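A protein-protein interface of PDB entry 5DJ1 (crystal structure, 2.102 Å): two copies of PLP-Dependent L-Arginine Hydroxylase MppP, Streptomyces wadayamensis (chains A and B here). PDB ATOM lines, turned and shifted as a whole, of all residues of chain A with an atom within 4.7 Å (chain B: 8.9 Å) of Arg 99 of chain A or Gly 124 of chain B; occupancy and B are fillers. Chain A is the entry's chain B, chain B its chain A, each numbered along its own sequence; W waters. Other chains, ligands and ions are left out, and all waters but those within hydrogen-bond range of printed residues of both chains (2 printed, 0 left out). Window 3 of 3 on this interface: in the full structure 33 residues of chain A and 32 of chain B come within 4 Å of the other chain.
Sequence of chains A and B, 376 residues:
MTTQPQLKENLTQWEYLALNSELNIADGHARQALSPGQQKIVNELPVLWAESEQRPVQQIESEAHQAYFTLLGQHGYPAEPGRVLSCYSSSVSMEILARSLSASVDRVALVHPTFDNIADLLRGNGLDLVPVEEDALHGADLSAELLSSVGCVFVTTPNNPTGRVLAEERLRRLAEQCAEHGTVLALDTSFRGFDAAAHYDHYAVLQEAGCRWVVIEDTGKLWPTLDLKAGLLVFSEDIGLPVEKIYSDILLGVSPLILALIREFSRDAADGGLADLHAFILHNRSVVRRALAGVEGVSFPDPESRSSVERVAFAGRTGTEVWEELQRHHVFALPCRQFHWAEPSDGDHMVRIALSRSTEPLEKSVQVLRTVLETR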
ATOM      1  N   GLU A  95       4.806 -25.578 -14.435  1.00  0.00           N
ATOM      2  CA  GLU A  95       5.845 -24.545 -14.521  1.00  0.00           C
ATOM      3  C   GLU A  95       5.234 -23.177 -14.835  1.00  0.00           C
ATOM      4  O   GLU A  95       5.615 -22.146 -14.246  1.00  0.00           O
ATOM      5  CB  GLU A  95       6.889 -24.945 -15.587  1.00  0.00           C
ATOM      6  CG  GLU A  95       7.938 -23.852 -15.975  1.00  0.00           C
ATOM      7  CD  GLU A  95       8.963 -23.563 -14.889  1.00  0.00           C
ATOM      8  OE1 GLU A  95       8.901 -24.229 -13.851  1.00  0.00           O
ATOM      9  OE2 GLU A  95       9.843 -22.668 -15.071  1.00  0.00           O
ATOM     10  N   ILE A  96       4.291 -23.143 -15.770  1.00  0.00           N
ATOM     11  CA  ILE A  96       3.604 -21.903 -16.107  1.00  0.00           C
ATOM     12  C   ILE A  96       2.853 -21.374 -14.898  1.00  0.00           C
ATOM     13  O   ILE A  96       2.924 -20.182 -14.573  1.00  0.00           O
ATOM     14  CB  ILE A  96       2.658 -22.125 -17.303  1.00  0.00           C
ATOM     15  CG1 ILE A  96       3.481 -22.321 -18.585  1.00  0.00           C
ATOM     16  CG2 ILE A  96       1.696 -20.983 -17.469  1.00  0.00           C
ATOM     17  CD1 ILE A  96       2.743 -23.060 -19.674  1.00  0.00           C
ATOM     18  N   LEU A  97       2.142 -22.256 -14.203  1.00  0.00           N
ATOM     19  CA  LEU A  97       1.384 -21.833 -13.042  1.00  0.00           C
ATOM     20  C   LEU A  97       2.318 -21.353 -11.923  1.00  0.00           C
ATOM     21  O   LEU A  97       2.095 -20.296 -11.330  1.00  0.00           O
ATOM     22  CB  LEU A  97       0.477 -22.968 -12.563  1.00  0.00           C
ATOM     23  CG  LEU A  97      -0.279 -22.690 -11.248  1.00  0.00           C
ATOM     24  CD1 LEU A  97      -1.208 -21.466 -11.378  1.00  0.00           C
ATOM     25  CD2 LEU A  97      -1.052 -23.930 -10.804  1.00  0.00           C
ATOM     26  N   ALA A  98       3.377 -22.111 -11.648  1.00  0.00           N
ATOM     27  CA  ALA A  98       4.300 -21.757 -10.573  1.00  0.00           C
ATOM     28  C   ALA A  98       4.937 -20.395 -10.826  1.00  0.00           C
ATOM     29  O   ALA A  98       4.942 -19.519  -9.957  1.00  0.00           O
ATOM     30  CB  ALA A  98       5.366 -22.835 -10.429  1.00  0.00           C
ATOM     31  N   ARG A  99       5.448 -20.179 -12.032  1.00  0.00           N
ATOM     32  CA  ARG A  99       6.064 -18.895 -12.314  1.00  0.00           C
ATOM     33  C   ARG A  99       5.028 -17.783 -12.288  1.00  0.00           C
ATOM     34  O   ARG A  99       5.311 -16.679 -11.794  1.00  0.00           O
ATOM     35  CB  ARG A  99       6.799 -18.928 -13.651  1.00  0.00           C
ATOM     36  CG  ARG A  99       7.586 -17.625 -13.878  1.00  0.00           C
ATOM     37  CD  ARG A  99       8.918 -17.872 -14.561  1.00  0.00           C
ATOM     38  NE  ARG A  99       8.844 -18.290 -15.953  1.00  0.00           N
ATOM     39  CZ  ARG A  99       8.469 -17.503 -16.966  1.00  0.00           C
ATOM     40  NH1 ARG A  99       8.077 -16.271 -16.751  1.00  0.00           N
ATOM     41  NH2 ARG A  99       8.531 -17.934 -18.215  1.00  0.00           N
ATOM     42  N   SER A 100       3.812 -18.070 -12.767  1.00  0.00           N
ATOM     43  CA  SER A 100       2.727 -17.091 -12.719  1.00  0.00           C
ATOM     44  C   SER A 100       2.409 -16.696 -11.282  1.00  0.00           C
ATOM     45  O   SER A 100       2.226 -15.523 -10.986  1.00  0.00           O
ATOM     46  CB  SER A 100       1.460 -17.640 -13.377  1.00  0.00           C
ATOM     47  OG  SER A 100       1.606 -17.785 -14.780  1.00  0.00           O
ATOM     48  N   LEU A 101       2.272 -17.681 -10.389  1.00  0.00           N
ATOM     49  CA  LEU A 101       2.032 -17.393  -8.979  1.00  0.00           C
ATOM     50  C   LEU A 101       3.100 -16.461  -8.409  1.00  0.00           C
ATOM     51  O   LEU A 101       2.789 -15.545  -7.635  1.00  0.00           O
ATOM     52  CB  LEU A 101       1.986 -18.710  -8.192  1.00  0.00           C
ATOM     53  CG  LEU A 101       0.677 -19.499  -8.271  1.00  0.00           C
ATOM     54  CD1 LEU A 101       0.870 -20.936  -7.735  1.00  0.00           C
ATOM     55  CD2 LEU A 101      -0.459 -18.770  -7.505  1.00  0.00           C
ATOM     56  N   SER A 102       4.367 -16.685  -8.763  1.00  0.00           N
ATOM     57  CA  SER A 102       5.448 -15.914  -8.137  1.00  0.00           C
ATOM     58  C   SER A 102       5.376 -14.428  -8.446  1.00  0.00           C
ATOM     59  O   SER A 102       6.091 -13.664  -7.815  1.00  0.00           O
ATOM     60  CB  SER A 102       6.845 -16.409  -8.546  1.00  0.00           C
ATOM     61  OG  SER A 102       7.102 -16.135  -9.897  1.00  0.00           O
ATOM     62  N   ALA A 103       4.553 -14.003  -9.398  1.00  0.00           N
ATOM     63  CA  ALA A 103       4.396 -12.579  -9.643  1.00  0.00           C
ATOM     64  C   ALA A 103       3.862 -11.862  -8.405  1.00  0.00           C
ATOM     65  O   ALA A 103       4.217 -10.710  -8.144  1.00  0.00           O
ATOM     66  CB  ALA A 103       3.458 -12.355 -10.830  1.00  0.00           C
ATOM     67  N   ASN A 125      10.518 -21.793  -8.344  1.00  0.00           N
ATOM     68  CA  ASN A 125      10.035 -20.499  -8.782  1.00  0.00           C
ATOM     69  C   ASN A 125       9.871 -19.514  -7.629  1.00  0.00           C
ATOM     70  O   ASN A 125       9.279 -18.450  -7.805  1.00  0.00           O
ATOM     71  CB  ASN A 125       8.729 -20.662  -9.550  1.00  0.00           C
ATOM     72  CG  ASN A 125       8.979 -21.115 -10.970  1.00  0.00           C
ATOM     73  OD1 ASN A 125       9.319 -20.315 -11.819  1.00  0.00           O
ATOM     74  ND2 ASN A 125       8.892 -22.403 -11.207  1.00  0.00           N
ATOM     75  N   ILE A 246       2.545 -15.997 -19.773  1.00  0.00           N
ATOM     76  CA  ILE A 246       3.648 -16.929 -19.594  1.00  0.00           C
ATOM     77  C   ILE A 246       3.433 -18.182 -20.446  1.00  0.00           C
ATOM     78  O   ILE A 246       4.381 -18.726 -21.017  1.00  0.00           O
ATOM     79  CB  ILE A 246       3.837 -17.233 -18.094  1.00  0.00           C
ATOM     80  CG1 ILE A 246       4.391 -15.969 -17.416  1.00  0.00           C
ATOM     81  CG2 ILE A 246       4.792 -18.384 -17.917  1.00  0.00           C
ATOM     82  CD1 ILE A 246       4.457 -16.032 -15.886  1.00  0.00           C
ATOM     83  N   ILE A 250       6.015 -19.544 -23.586  1.00  0.00           N
ATOM     84  CA  ILE A 250       6.585 -20.879 -23.710  1.00  0.00           C
ATOM     85  C   ILE A 250       6.072 -21.623 -24.955  1.00  0.00           C
ATOM     86  O   ILE A 250       6.826 -22.394 -25.560  1.00  0.00           O
ATOM     87  CB  ILE A 250       6.327 -21.674 -22.411  1.00  0.00           C
ATOM     88  CG1 ILE A 250       7.124 -21.028 -21.270  1.00  0.00           C
ATOM     89  CG2 ILE A 250       6.705 -23.173 -22.600  1.00  0.00           C
ATOM     90  CD1 ILE A 250       6.951 -21.654 -19.945  1.00  0.00           C
ATOM     91  N   SER B  91      11.664 -23.727 -26.796  1.00  0.00           N
ATOM     92  CA  SER B  91      11.262 -22.755 -25.789  1.00  0.00           C
ATOM     93  C   SER B  91      11.201 -23.396 -24.409  1.00  0.00           C
ATOM     94  O   SER B  91      11.473 -22.719 -23.419  1.00  0.00           O
ATOM     95  CB  SER B  91       9.899 -22.115 -26.147  1.00  0.00           C
ATOM     96  OG  SER B  91      10.002 -21.321 -27.334  1.00  0.00           O
ATOM     97  N   MET B  94      14.634 -23.307 -23.358  1.00  0.00           N
ATOM     98  CA  MET B  94      14.992 -21.936 -23.024  1.00  0.00           C
ATOM     99  C   MET B  94      14.450 -21.562 -21.646  1.00  0.00           C
ATOM    100  O   MET B  94      15.138 -20.876 -20.882  1.00  0.00           O
ATOM    101  CB  MET B  94      14.473 -20.997 -24.123  1.00  0.00           C
ATOM    102  CG  MET B  94      14.893 -19.527 -23.915  1.00  0.00           C
ATOM    103  SD  MET B  94      16.676 -19.228 -24.207  1.00  0.00           S
ATOM    104  CE  MET B  94      16.995 -18.484 -22.689  1.00  0.00           C
ATOM    105  N   GLU B  95      13.253 -22.064 -21.287  1.00  0.00           N
ATOM    106  CA  GLU B  95      12.727 -21.848 -19.939  1.00  0.00           C
ATOM    107  C   GLU B  95      13.638 -22.463 -18.899  1.00  0.00           C
ATOM    108  O   GLU B  95      13.938 -21.836 -17.872  1.00  0.00           O
ATOM    109  CB  GLU B  95      11.283 -22.409 -19.823  1.00  0.00           C
ATOM    110  CG  GLU B  95      10.694 -22.455 -18.399  1.00  0.00           C
ATOM    111  CD  GLU B  95      10.307 -21.060 -17.860  1.00  0.00           C
ATOM    112  OE1 GLU B  95      10.488 -20.047 -18.583  1.00  0.00           O
ATOM    113  OE2 GLU B  95       9.803 -20.994 -16.721  1.00  0.00           O
ATOM    114  N   ILE B  96      14.112 -23.683 -19.165  1.00  0.00           N
ATOM    115  CA  ILE B  96      15.039 -24.362 -18.273  1.00  0.00           C
ATOM    116  C   ILE B  96      16.310 -23.535 -18.113  1.00  0.00           C
ATOM    117  O   ILE B  96      16.791 -23.298 -17.003  1.00  0.00           O
ATOM    118  CB  ILE B  96      15.324 -25.785 -18.809  1.00  0.00           C
ATOM    119  CG1 ILE B  96      14.087 -26.678 -18.635  1.00  0.00           C
ATOM    120  CG2 ILE B  96      16.498 -26.422 -18.106  1.00  0.00           C
ATOM    121  CD1 ILE B  96      14.081 -27.892 -19.578  1.00  0.00           C
ATOM    122  N   ALA B  98      16.796 -20.338 -18.766  1.00  0.00           N
ATOM    123  CA  ALA B  98      16.579 -19.022 -18.158  1.00  0.00           C
ATOM    124  C   ALA B  98      16.419 -19.151 -16.651  1.00  0.00           C
ATOM    125  O   ALA B  98      17.029 -18.386 -15.879  1.00  0.00           O
ATOM    126  CB  ALA B  98      15.355 -18.330 -18.781  1.00  0.00           C
ATOM    127  N   ARG B  99      15.638 -20.142 -16.203  1.00  0.00           N
ATOM    128  CA  ARG B  99      15.484 -20.300 -14.761  1.00  0.00           C
ATOM    129  C   ARG B  99      16.796 -20.729 -14.132  1.00  0.00           C
ATOM    130  O   ARG B  99      17.141 -20.269 -13.045  1.00  0.00           O
ATOM    131  CB  ARG B  99      14.356 -21.272 -14.421  1.00  0.00           C
ATOM    132  CG  ARG B  99      14.105 -21.338 -12.934  1.00  0.00           C
ATOM    133  CD  ARG B  99      12.657 -21.409 -12.585  1.00  0.00           C
ATOM    134  NE  ARG B  99      12.014 -22.704 -12.900  1.00  0.00           N
ATOM    135  CZ  ARG B  99      12.219 -23.852 -12.270  1.00  0.00           C
ATOM    136  NH1 ARG B  99      13.107 -23.961 -11.304  1.00  0.00           N
ATOM    137  NH2 ARG B  99      11.488 -24.909 -12.591  1.00  0.00           N
ATOM    138  N   SER B 102      19.076 -17.682 -13.653  1.00  0.00           N
ATOM    139  CA  SER B 102      18.627 -16.833 -12.562  1.00  0.00           C
ATOM    140  C   SER B 102      19.180 -17.280 -11.213  1.00  0.00           C
ATOM    141  O   SER B 102      19.149 -16.485 -10.285  1.00  0.00           O
ATOM    142  CB  SER B 102      17.079 -16.751 -12.487  1.00  0.00           C
ATOM    143  OG  SER B 102      16.502 -17.924 -11.969  1.00  0.00           O
ATOM    144  N   ASP B 116      11.702 -12.964 -30.076  1.00  0.00           N
ATOM    145  CA  ASP B 116      11.405 -12.183 -28.870  1.00  0.00           C
ATOM    146  C   ASP B 116      11.092 -13.069 -27.668  1.00  0.00           C
ATOM    147  O   ASP B 116      11.333 -12.653 -26.535  1.00  0.00           O
ATOM    148  CB  ASP B 116      10.253 -11.186 -29.112  1.00  0.00           C
ATOM    149  CG  ASP B 116       9.090 -11.789 -29.865  1.00  0.00           C
ATOM    150  OD1 ASP B 116       9.259 -12.116 -31.068  1.00  0.00           O
ATOM    151  OD2 ASP B 116       8.002 -11.902 -29.263  1.00  0.00           O
ATOM    152  N   ASN B 117      10.610 -14.292 -27.891  1.00  0.00           N
ATOM    153  CA  ASN B 117      10.365 -15.208 -26.774  1.00  0.00           C
ATOM    154  C   ASN B 117      11.590 -15.376 -25.911  1.00  0.00           C
ATOM    155  O   ASN B 117      11.456 -15.627 -24.718  1.00  0.00           O
ATOM    156  CB  ASN B 117       9.920 -16.599 -27.247  1.00  0.00           C
ATOM    157  CG  ASN B 117       8.525 -16.596 -27.872  1.00  0.00           C
ATOM    158  OD1 ASN B 117       8.293 -15.974 -28.898  1.00  0.00           O
ATOM    159  ND2 ASN B 117       7.602 -17.317 -27.252  1.00  0.00           N
ATOM    160  N   ILE B 118      12.782 -15.302 -26.499  1.00  0.00           N
ATOM    161  CA  ILE B 118      14.002 -15.464 -25.718  1.00  0.00           C
ATOM    162  C   ILE B 118      14.105 -14.352 -24.686  1.00  0.00           C
ATOM    163  O   ILE B 118      14.412 -14.593 -23.511  1.00  0.00           O
ATOM    164  CB  ILE B 118      15.236 -15.485 -26.642  1.00  0.00           C
ATOM    165  CG1 ILE B 118      15.186 -16.716 -27.588  1.00  0.00           C
ATOM    166  CG2 ILE B 118      16.507 -15.476 -25.803  1.00  0.00           C
ATOM    167  CD1 ILE B 118      16.210 -16.664 -28.737  1.00  0.00           C
ATOM    168  N   ALA B 119      13.894 -13.107 -25.132  1.00  0.00           N
ATOM    169  CA  ALA B 119      13.865 -11.985 -24.198  1.00  0.00           C
ATOM    170  C   ALA B 119      12.747 -12.158 -23.174  1.00  0.00           C
ATOM    171  O   ALA B 119      12.940 -11.895 -21.982  1.00  0.00           O
ATOM    172  CB  ALA B 119      13.685 -10.668 -24.942  1.00  0.00           C
ATOM    173  N   ASP B 120      11.569 -12.598 -23.615  1.00  0.00           N
ATOM    174  CA  ASP B 120      10.457 -12.748 -22.675  1.00  0.00           C
ATOM    175  C   ASP B 120      10.753 -13.801 -21.617  1.00  0.00           C
ATOM    176  O   ASP B 120      10.392 -13.618 -20.446  1.00  0.00           O
ATOM    177  CB  ASP B 120       9.157 -13.110 -23.390  1.00  0.00           C
ATOM    178  CG  ASP B 120       8.661 -11.998 -24.311  1.00  0.00           C
ATOM    179  OD1 ASP B 120       9.024 -10.809 -24.103  1.00  0.00           O
ATOM    180  OD2 ASP B 120       7.963 -12.343 -25.290  1.00  0.00           O
ATOM    181  N   LEU B 121      11.368 -14.919 -22.007  1.00  0.00           N
ATOM    182  CA  LEU B 121      11.686 -15.963 -21.032  1.00  0.00           C
ATOM    183  C   LEU B 121      12.807 -15.539 -20.081  1.00  0.00           C
ATOM    184  O   LEU B 121      12.724 -15.796 -18.869  1.00  0.00           O
ATOM    185  CB  LEU B 121      12.010 -17.278 -21.747  1.00  0.00           C
ATOM    186  CG  LEU B 121      10.832 -17.876 -22.523  1.00  0.00           C
ATOM    187  CD1 LEU B 121      11.230 -19.042 -23.412  1.00  0.00           C
ATOM    188  CD2 LEU B 121       9.719 -18.304 -21.604  1.00  0.00           C
ATOM    189  N   LEU B 122      13.839 -14.861 -20.586  1.00  0.00           N
ATOM    190  CA  LEU B 122      14.885 -14.333 -19.711  1.00  0.00           C
ATOM    191  C   LEU B 122      14.333 -13.294 -18.729  1.00  0.00           C
ATOM    192  O   LEU B 122      14.565 -13.386 -17.518  1.00  0.00           O
ATOM    193  CB  LEU B 122      16.012 -13.754 -20.567  1.00  0.00           C
ATOM    194  CG  LEU B 122      16.869 -14.810 -21.285  1.00  0.00           C
ATOM    195  CD1 LEU B 122      17.717 -14.169 -22.373  1.00  0.00           C
ATOM    196  CD2 LEU B 122      17.772 -15.539 -20.313  1.00  0.00           C
ATOM    197  N   ARG B 123      13.608 -12.294 -19.242  1.00  0.00           N
ATOM    198  CA  ARG B 123      13.016 -11.267 -18.389  1.00  0.00           C
ATOM    199  C   ARG B 123      12.067 -11.876 -17.365  1.00  0.00           C
ATOM    200  O   ARG B 123      12.063 -11.477 -16.192  1.00  0.00           O
ATOM    201  CB  ARG B 123      12.290 -10.230 -19.261  1.00  0.00           C
ATOM    202  CG  ARG B 123      11.575  -9.143 -18.516  1.00  0.00           C
ATOM    203  CD  ARG B 123      10.560  -8.400 -19.423  1.00  0.00           C
ATOM    204  NE  ARG B 123      11.154  -7.947 -20.692  1.00  0.00           N
ATOM    205  CZ  ARG B 123      10.858  -8.439 -21.897  1.00  0.00           C
ATOM    206  NH1 ARG B 123       9.944  -9.400 -22.035  1.00  0.00           N
ATOM    207  NH2 ARG B 123      11.475  -7.968 -22.986  1.00  0.00           N
ATOM    208  N   GLY B 124      11.243 -12.833 -17.794  1.00  0.00           N
ATOM    209  CA  GLY B 124      10.262 -13.430 -16.894  1.00  0.00           C
ATOM    210  C   GLY B 124      10.888 -14.221 -15.758  1.00  0.00           C
ATOM    211  O   GLY B 124      10.270 -14.400 -14.712  1.00  0.00           O
ATOM    212  N   ASN B 125      12.100 -14.704 -15.948  1.00  0.00           N
ATOM    213  CA  ASN B 125      12.831 -15.401 -14.910  1.00  0.00           C
ATOM    214  C   ASN B 125      13.753 -14.473 -14.139  1.00  0.00           C
ATOM    215  O   ASN B 125      14.557 -14.945 -13.347  1.00  0.00           O
ATOM    216  CB  ASN B 125      13.589 -16.564 -15.525  1.00  0.00           C
ATOM    217  CG  ASN B 125      12.707 -17.759 -15.736  1.00  0.00           C
ATOM    218  OD1 ASN B 125      12.484 -18.512 -14.821  1.00  0.00           O
ATOM    219  ND2 ASN B 125      12.212 -17.940 -16.943  1.00  0.00           N
ATOM    220  N   GLY B 126      13.600 -13.164 -14.303  1.00  0.00           N
ATOM    221  CA  GLY B 126      14.278 -12.213 -13.452  1.00  0.00           C
ATOM    222  C   GLY B 126      15.587 -11.666 -13.981  1.00  0.00           C
ATOM    223  O   GLY B 126      16.257 -10.930 -13.264  1.00  0.00           O
ATOM    224  N   LEU B 127      15.959 -11.959 -15.223  1.00  0.00           N
ATOM    225  CA  LEU B 127      17.208 -11.435 -15.757  1.00  0.00           C
ATOM    226  C   LEU B 127      16.997 -10.044 -16.345  1.00  0.00           C
ATOM    227  O   LEU B 127      16.007  -9.799 -17.042  1.00  0.00           O
ATOM    228  CB  LEU B 127      17.773 -12.371 -16.834  1.00  0.00           C
ATOM    229  CG  LEU B 127      18.335 -13.755 -16.433  1.00  0.00           C
ATOM    230  CD1 LEU B 127      19.302 -13.624 -15.254  1.00  0.00           C
ATOM    231  CD2 LEU B 127      17.285 -14.756 -16.097  1.00  0.00           C
ATOM    232  N   ASP B 128      17.934  -9.139 -16.064  1.00  0.00           N
ATOM    233  CA  ASP B 128      18.031  -7.867 -16.797  1.00  0.00           C
ATOM    234  C   ASP B 128      18.715  -8.111 -18.155  1.00  0.00           C
ATOM    235  O   ASP B 128      19.608  -8.959 -18.269  1.00  0.00           O
ATOM    236  CB  ASP B 128      18.833  -6.830 -15.981  1.00  0.00           C
ATOM    237  CG  ASP B 128      18.048  -6.260 -14.790  1.00  0.00           C
ATOM    238  OD1 ASP B 128      16.859  -5.890 -14.965  1.00  0.00           O
ATOM    239  OD2 ASP B 128      18.628  -6.180 -13.685  1.00  0.00           O
ATOM    240  N   LEU B 129      18.301  -7.383 -19.189  1.00  0.00           N
ATOM    241  CA  LEU B 129      18.775  -7.653 -20.548  1.00  0.00           C
ATOM    242  C   LEU B 129      19.583  -6.460 -21.060  1.00  0.00           C
ATOM    243  O   LEU B 129      19.196  -5.309 -20.856  1.00  0.00           O
ATOM    244  CB  LEU B 129      17.629  -7.950 -21.498  1.00  0.00           C
ATOM    245  CG  LEU B 129      16.771  -9.158 -21.124  1.00  0.00           C
ATOM    246  CD1 LEU B 129      15.549  -9.214 -21.994  1.00  0.00           C
ATOM    247  CD2 LEU B 129      17.590 -10.432 -21.240  1.00  0.00           C
ATOM    248  N   ILE B 250      10.854 -30.541 -14.912  1.00  0.00           N
ATOM    249  CA  ILE B 250       9.857 -30.283 -15.951  1.00  0.00           C
ATOM    250  C   ILE B 250       9.495 -31.557 -16.744  1.00  0.00           C
ATOM    251  O   ILE B 250       8.323 -31.762 -17.075  1.00  0.00           O
ATOM    252  CB  ILE B 250      10.365 -29.131 -16.851  1.00  0.00           C
ATOM    253  CG1 ILE B 250      10.382 -27.817 -16.019  1.00  0.00           C
ATOM    254  CG2 ILE B 250       9.486 -28.946 -18.140  1.00  0.00           C
ATOM    255  CD1 ILE B 250      10.969 -26.645 -16.696  1.00  0.00           C
HETATM  256  O   HOH W   1       8.088 -15.330 -19.693  1.00  0.00           O
HETATM  257  O   HOH W   2       7.573 -14.287 -14.763  1.00  0.00           O
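Of the 12 printed residues of chain A, 4 touch a printed residue of chain B. Hydrophobic or aromatic side chains of chain B that line the printed part of chain A: Leu 121. Among the printed residues, 10 pairs touch across the chains.
Arg 99 of chain A touches just these residues of chain B: Glu 95, Leu 121, Gly 124 and Asn 125. Gly 124 of chain B touches just one residue of chain A: Arg 99 (3.5 Å). No residue of chain B comes within 4 Å of Ser 100 of chain A. Printed residues of chain B within 4 Å of Asn 125 of chain A: Arg 99 (3.6 Å). Of the printed residues of chain A, Arg 99 of chain B touches Glu 95 and Asn 125. Of the printed residues of chain A, Glu 95 of chain B touches Glu 95, Arg 99 and Ile 250. Printed residues of chain B within 4 Å of Glu 95 of chain A: Glu 95 and Arg 99. Of the printed residues of chain A, Leu 121 of chain B touches Arg 99 and Ile 250.
Water W2 bridges O of Gly 124 of chain B (2.7 Å) and NH1 of Arg 99 of chain A (2.9 Å). Water W1 lies within hydrogen-bond range of the backbone carbonyl oxygen of Asp 120 of chain B (3.0 Å) and the guanidinium group of Arg 99 of chain A (3.0 Å).
The side-chain carboxylate (OE1) of Glu 95 of chain B lies within hydrogen-bond range of the side-chain amide nitrogen (ND2) of Asn 125 of chain B, 3.2 Å away. The backbone carbonyl oxygen of Arg 99 of chain B sits at hydrogen-bond distance from the side-chain hydroxyl of Ser 102 of chain B (2.7 Å). O of Leu 121 of chain B sits at hydrogen-bond distance from ND2 of Asn 125 of chain B, at 2.9 Å. The side-chain carboxylate (OE1) of Glu 95 of chain A is in hydrogen-bond range of the side-chain amide nitrogen (ND2) of Asn 125 of chain A (3.2 Å). The backbone carbonyl oxygen of Arg 99 of chain A sits at hydrogen-bond distance from the side-chain hydroxyl of Ser 102 of chain A.
The guanidinium group (NH2) of Arg 99 of chain A is in salt-bridge range of the side-chain carboxylate (OE1) of Glu 95 of chain B. The guanidinium group (NH2) of Arg 99 of chain B lies within salt-bridge range of the side-chain carboxylate (OE1) of Glu 95 of chain A, 3.0 Å away. The side-chain carboxylate (OE2) of Glu 95 of chain A lies close to the side-chain carboxylate (OE2) of Glu 95 of chain B (2.4 Å).
NH2 of Arg 99 of chain A touches CD2 of Leu 121 of chain B, 3.6 Å away. NH1 of Arg 99 of chain A touches O of Gly 124 of chain B, 3.5 Å away. NE of Arg 99 of chain A touches ND2 of Asn 125 of chain B, at 3.5 Å. Asn 125 of chain A touches Arg 99 of chain B. Ile 250 of chain A touches Ser 91 of chain B (O to CB, 3.1 Å). Glu 95 of chain B touches Ile 250 of chain A (CD to CD1, 3.995 Å). Leu 121 of chain B touches Ile 250 of chain A (CD2 to CG1, 3.8 Å).
Glu 95 of chain A touches its own counterpart, Glu 95 of chain B. Glu 95 of chain A touches Arg 99 of chain B, and with the chains exchanged Arg 99 of chain A touches Glu 95 of chain B. Arg 99 of chain A touches Asn 125 of chain B, and with the chains exchanged Asn 125 of chain A touches Arg 99 of chain B. Ile 250 of chain A touches Glu 95 of chain B, but with the chains exchanged Glu 95 of chain A does not touch Ile 250 of chain B (4.1 Å). 7 positions are printed for both chains. Of the 10 pairs that touch across the chains among the printed residues, 5 have their exchanged pair printed and touching as well.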
